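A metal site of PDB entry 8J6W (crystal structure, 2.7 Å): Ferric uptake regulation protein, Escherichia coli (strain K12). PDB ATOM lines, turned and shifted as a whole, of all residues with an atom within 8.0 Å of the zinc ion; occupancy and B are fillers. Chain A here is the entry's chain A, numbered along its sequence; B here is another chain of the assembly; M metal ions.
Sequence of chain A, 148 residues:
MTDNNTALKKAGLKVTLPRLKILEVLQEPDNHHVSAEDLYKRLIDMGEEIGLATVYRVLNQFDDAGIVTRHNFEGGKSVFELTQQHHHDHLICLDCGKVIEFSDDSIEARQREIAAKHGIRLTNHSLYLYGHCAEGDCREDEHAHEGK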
ATOM      1  N   HIS A  87      17.977   4.917 -30.845  1.00  0.00           N
ATOM      2  CA  HIS A  87      19.247   4.795 -30.130  1.00  0.00           C
ATOM      3  C   HIS A  87      19.078   3.976 -28.859  1.00  0.00           C
ATOM      4  O   HIS A  87      18.182   4.219 -28.049  1.00  0.00           O
ATOM      5  CB  HIS A  87      19.825   6.146 -29.738  1.00  0.00           C
ATOM      6  CG  HIS A  87      21.124   6.034 -29.015  1.00  0.00           C
ATOM      7  ND1 HIS A  87      22.298   5.680 -29.648  1.00  0.00           N
ATOM      8  CD2 HIS A  87      21.438   6.179 -27.702  1.00  0.00           C
ATOM      9  CE1 HIS A  87      23.278   5.645 -28.762  1.00  0.00           C
ATOM     10  NE2 HIS A  87      22.782   5.949 -27.578  1.00  0.00           N
ATOM     11  N   HIS A  88      19.981   3.027 -28.680  1.00  0.00           N
ATOM     12  CA  HIS A  88      20.064   2.311 -27.417  1.00  0.00           C
ATOM     13  C   HIS A  88      21.539   2.035 -27.152  1.00  0.00           C
ATOM     14  O   HIS A  88      22.388   2.236 -28.010  1.00  0.00           O
ATOM     15  CB  HIS A  88      19.248   1.023 -27.467  1.00  0.00           C
ATOM     16  CG  HIS A  88      19.646   0.104 -28.572  1.00  0.00           C
ATOM     17  ND1 HIS A  88      18.835  -0.151 -29.654  1.00  0.00           N
ATOM     18  CD2 HIS A  88      20.784  -0.598 -28.782  1.00  0.00           C
ATOM     19  CE1 HIS A  88      19.444  -1.000 -30.463  1.00  0.00           C
ATOM     20  NE2 HIS A  88      20.623  -1.281 -29.959  1.00  0.00           N
ATOM     21  N   ASP A  89      21.820   1.576 -25.947  1.00  0.00           N
ATOM     22  CA  ASP A  89      23.143   1.100 -25.592  1.00  0.00           C
ATOM     23  C   ASP A  89      23.007  -0.386 -25.277  1.00  0.00           C
ATOM     24  O   ASP A  89      21.960  -0.989 -25.528  1.00  0.00           O
ATOM     25  CB  ASP A  89      23.716   1.947 -24.463  1.00  0.00           C
ATOM     26  CG  ASP A  89      24.086   3.347 -24.924  1.00  0.00           C
ATOM     27  OD1 ASP A  89      24.925   3.495 -25.851  1.00  0.00           O
ATOM     28  OD2 ASP A  89      23.478   4.287 -24.391  1.00  0.00           O
ATOM     29  N   HIS A  90      24.060  -0.992 -24.750  1.00  0.00           N
ATOM     30  CA  HIS A  90      24.105  -2.450 -24.703  1.00  0.00           C
ATOM     31  C   HIS A  90      24.502  -2.961 -23.332  1.00  0.00           C
ATOM     32  O   HIS A  90      25.535  -2.551 -22.794  1.00  0.00           O
ATOM     33  CB  HIS A  90      25.050  -3.001 -25.763  1.00  0.00           C
ATOM     34  CG  HIS A  90      24.707  -2.555 -27.143  1.00  0.00           C
ATOM     35  ND1 HIS A  90      25.316  -1.485 -27.756  1.00  0.00           N
ATOM     36  CD2 HIS A  90      23.814  -3.042 -28.040  1.00  0.00           C
ATOM     37  CE1 HIS A  90      24.818  -1.330 -28.964  1.00  0.00           C
ATOM     38  NE2 HIS A  90      23.920  -2.265 -29.168  1.00  0.00           N
ATOM     39  N   PHE A 102      18.976  -0.969 -24.125  1.00  0.00           N
ATOM     40  CA  PHE A 102      18.464  -0.076 -23.098  1.00  0.00           C
ATOM     41  C   PHE A 102      18.772   1.361 -23.490  1.00  0.00           C
ATOM     42  O   PHE A 102      19.763   1.647 -24.175  1.00  0.00           O
ATOM     43  CB  PHE A 102      19.035  -0.376 -21.694  1.00  0.00           C
ATOM     44  CG  PHE A 102      20.484   0.066 -21.470  1.00  0.00           C
ATOM     45  CD1 PHE A 102      20.799   1.351 -21.053  1.00  0.00           C
ATOM     46  CD2 PHE A 102      21.519  -0.849 -21.599  1.00  0.00           C
ATOM     47  CE1 PHE A 102      22.115   1.746 -20.853  1.00  0.00           C
ATOM     48  CE2 PHE A 102      22.844  -0.473 -21.385  1.00  0.00           C
ATOM     49  CZ  PHE A 102      23.137   0.828 -21.015  1.00  0.00           C
ATOM     50  N   SER A 103      17.907   2.266 -23.042  1.00  0.00           N
ATOM     51  CA  SER A 103      18.124   3.680 -23.242  1.00  0.00           C
ATOM     52  C   SER A 103      17.671   4.400 -21.986  1.00  0.00           C
ATOM     53  O   SER A 103      16.594   4.102 -21.442  1.00  0.00           O
ATOM     54  CB  SER A 103      17.383   4.217 -24.479  1.00  0.00           C
ATOM     55  OG  SER A 103      17.561   5.622 -24.585  1.00  0.00           O
ATOM     56  N   ASP A 104      18.507   5.317 -21.510  1.00  0.00           N
ATOM     57  CA  ASP A 104      18.271   6.087 -20.298  1.00  0.00           C
ATOM     58  C   ASP A 104      18.341   7.555 -20.707  1.00  0.00           C
ATOM     59  O   ASP A 104      19.356   7.991 -21.262  1.00  0.00           O
ATOM     60  CB  ASP A 104      19.311   5.732 -19.224  1.00  0.00           C
ATOM     61  CG  ASP A 104      18.887   6.134 -17.811  1.00  0.00           C
ATOM     62  OD1 ASP A 104      18.667   7.351 -17.575  1.00  0.00           O
ATOM     63  OD2 ASP A 104      18.804   5.241 -16.931  1.00  0.00           O
ATOM     64  N   ILE A 107      20.908   9.597 -18.609  1.00  0.00           N
ATOM     65  CA  ILE A 107      22.309   9.384 -18.965  1.00  0.00           C
ATOM     66  C   ILE A 107      22.646  10.107 -20.268  1.00  0.00           C
ATOM     67  O   ILE A 107      23.613  10.858 -20.328  1.00  0.00           O
ATOM     68  CB  ILE A 107      22.625   7.884 -19.065  1.00  0.00           C
ATOM     69  CG1 ILE A 107      22.482   7.208 -17.700  1.00  0.00           C
ATOM     70  CG2 ILE A 107      24.050   7.679 -19.584  1.00  0.00           C
ATOM     71  CD1 ILE A 107      22.992   5.772 -17.673  1.00  0.00           C
ATOM     72  N   GLU A 108      21.848   9.898 -21.318  1.00  0.00           N
ATOM     73  CA  GLU A 108      22.112  10.571 -22.584  1.00  0.00           C
ATOM     74  C   GLU A 108      22.172  12.085 -22.394  1.00  0.00           C
ATOM     75  O   GLU A 108      22.845  12.781 -23.158  1.00  0.00           O
ATOM     76  CB  GLU A 108      21.051  10.235 -23.651  1.00  0.00           C
ATOM     77  CG  GLU A 108      20.781   8.740 -23.857  1.00  0.00           C
ATOM     78  CD  GLU A 108      21.905   7.967 -24.568  1.00  0.00           C
ATOM     79  OE1 GLU A 108      22.521   8.484 -25.528  1.00  0.00           O
ATOM     80  OE2 GLU A 108      22.158   6.811 -24.185  1.00  0.00           O
ATOM     81  N   GLN A 111      25.552  12.908 -20.455  1.00  0.00           N
ATOM     82  CA  GLN A 111      26.633  12.742 -21.418  1.00  0.00           C
ATOM     83  C   GLN A 111      26.802  14.005 -22.249  1.00  0.00           C
ATOM     84  O   GLN A 111      27.927  14.472 -22.472  1.00  0.00           O
ATOM     85  CB  GLN A 111      26.366  11.545 -22.300  1.00  0.00           C
ATOM     86  CG  GLN A 111      26.615  10.210 -21.632  1.00  0.00           C
ATOM     87  CD  GLN A 111      26.230   9.023 -22.511  1.00  0.00           C
ATOM     88  OE1 GLN A 111      25.680   9.195 -23.601  1.00  0.00           O
ATOM     89  NE2 GLN A 111      26.491   7.820 -22.027  1.00  0.00           N
ATOM     90  N   LEU A 122      28.802  16.824 -27.987  1.00  0.00           N
ATOM     91  CA  LEU A 122      28.740  15.381 -28.135  1.00  0.00           C
ATOM     92  C   LEU A 122      28.135  14.981 -29.458  1.00  0.00           C
ATOM     93  O   LEU A 122      26.986  15.336 -29.753  1.00  0.00           O
ATOM     94  CB  LEU A 122      27.906  14.784 -26.994  1.00  0.00           C
ATOM     95  CG  LEU A 122      27.956  13.263 -26.925  1.00  0.00           C
ATOM     96  CD1 LEU A 122      29.365  12.790 -26.442  1.00  0.00           C
ATOM     97  CD2 LEU A 122      26.899  12.831 -25.972  1.00  0.00           C
ATOM     98  N   ASN A 124      28.981  11.428 -30.868  1.00  0.00           N
ATOM     99  CA  ASN A 124      28.783   9.989 -30.844  1.00  0.00           C
ATOM    100  C   ASN A 124      29.276   9.451 -29.507  1.00  0.00           C
ATOM    101  O   ASN A 124      30.006  10.134 -28.776  1.00  0.00           O
ATOM    102  CB  ASN A 124      29.504   9.320 -32.017  1.00  0.00           C
ATOM    103  CG  ASN A 124      29.140   7.852 -32.176  1.00  0.00           C
ATOM    104  OD1 ASN A 124      28.043   7.430 -31.814  1.00  0.00           O
ATOM    105  ND2 ASN A 124      30.048   7.077 -32.743  1.00  0.00           N
ATOM    106  N   HIS A 125      28.853   8.233 -29.197  1.00  0.00           N
ATOM    107  CA  HIS A 125      29.232   7.604 -27.944  1.00  0.00           C
ATOM    108  C   HIS A 125      28.918   6.129 -28.026  1.00  0.00           C
ATOM    109  O   HIS A 125      28.050   5.708 -28.792  1.00  0.00           O
ATOM    110  CB  HIS A 125      28.519   8.244 -26.750  1.00  0.00           C
ATOM    111  CG  HIS A 125      27.049   8.014 -26.721  1.00  0.00           C
ATOM    112  ND1 HIS A 125      26.160   8.766 -27.455  1.00  0.00           N
ATOM    113  CD2 HIS A 125      26.298   7.112 -26.039  1.00  0.00           C
ATOM    114  CE1 HIS A 125      24.928   8.335 -27.239  1.00  0.00           C
ATOM    115  NE2 HIS A 125      24.988   7.336 -26.386  1.00  0.00           N
ATOM    116  N   SER A 126      29.638   5.344 -27.236  1.00  0.00           N
ATOM    117  CA  SER A 126      29.318   3.937 -27.073  1.00  0.00           C
ATOM    118  C   SER A 126      29.405   3.584 -25.607  1.00  0.00           C
ATOM    119  O   SER A 126      30.362   3.957 -24.909  1.00  0.00           O
ATOM    120  CB  SER A 126      30.215   3.036 -27.924  1.00  0.00           C
ATOM    121  OG  SER A 126      31.498   2.908 -27.385  1.00  0.00           O
ATOM    122  N   LEU A 127      28.385   2.874 -25.134  1.00  0.00           N
ATOM    123  CA  LEU A 127      28.285   2.510 -23.739  1.00  0.00           C
ATOM    124  C   LEU A 127      28.011   1.020 -23.692  1.00  0.00           C
ATOM    125  O   LEU A 127      26.947   0.580 -24.101  1.00  0.00           O
ATOM    126  CB  LEU A 127      27.193   3.317 -23.035  1.00  0.00           C
ATOM    127  CG  LEU A 127      26.752   2.902 -21.635  1.00  0.00           C
ATOM    128  CD1 LEU A 127      27.915   2.727 -20.675  1.00  0.00           C
ATOM    129  CD2 LEU A 127      25.818   3.982 -21.154  1.00  0.00           C
ATOM    130  N   LEU B 127      32.701   3.309 -21.300  1.00  0.00           N
ATOM    131  CA  LEU B 127      31.895   4.417 -21.760  1.00  0.00           C
ATOM    132  C   LEU B 127      32.827   5.366 -22.486  1.00  0.00           C
ATOM    133  O   LEU B 127      33.686   5.975 -21.865  1.00  0.00           O
ATOM    134  CB  LEU B 127      31.176   5.099 -20.595  1.00  0.00           C
ATOM    135  CG  LEU B 127      30.490   6.440 -20.830  1.00  0.00           C
ATOM    136  CD1 LEU B 127      29.557   6.425 -22.029  1.00  0.00           C
ATOM    137  CD2 LEU B 127      29.732   6.749 -19.566  1.00  0.00           C
ATOM    138  N   LEU B 129      32.969   8.719 -24.927  1.00  0.00           N
ATOM    139  CA  LEU B 129      32.265   9.858 -25.473  1.00  0.00           C
ATOM    140  C   LEU B 129      33.112  10.489 -26.559  1.00  0.00           C
ATOM    141  O   LEU B 129      34.324  10.645 -26.407  1.00  0.00           O
ATOM    142  CB  LEU B 129      31.945  10.904 -24.392  1.00  0.00           C
ATOM    143  CG  LEU B 129      31.013  10.485 -23.249  1.00  0.00           C
ATOM    144  CD1 LEU B 129      30.680  11.654 -22.348  1.00  0.00           C
ATOM    145  CD2 LEU B 129      29.743   9.828 -23.786  1.00  0.00           C
HETATM  146 ZN    ZN M   1      23.537   5.928 -25.435  1.00  0.00          ZN
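Along chain A the residues within 4 Å of the zinc ion span positions 87 to 125.
OD2 of Asp 89 binds the zinc ion (1.9 Å). The side-chain carboxylate (OE2) of Glu 108 binds the zinc ion. NE2 of His 125 binds the zinc ion, at 2.2 Å. NE2 of His 87 is bound to the zinc ion, at 2.3 Å. The zinc ion has four donor atoms within binding distance. Slightly farther from the zinc ion lies OE1 of Glu 108 (2.8 Å). Slightly farther from the zinc ion lies the side-chain carboxylate (OD1) of Asp 89 (2.8 Å).
N of Asp 89 lies within hydrogen-bond range of O of Phe 102, at 2.7 Å. The side-chain amide oxygen (OE1) of Gln 111 lies close to a ring nitrogen (NE2) of His 125, 3.4 Å away.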
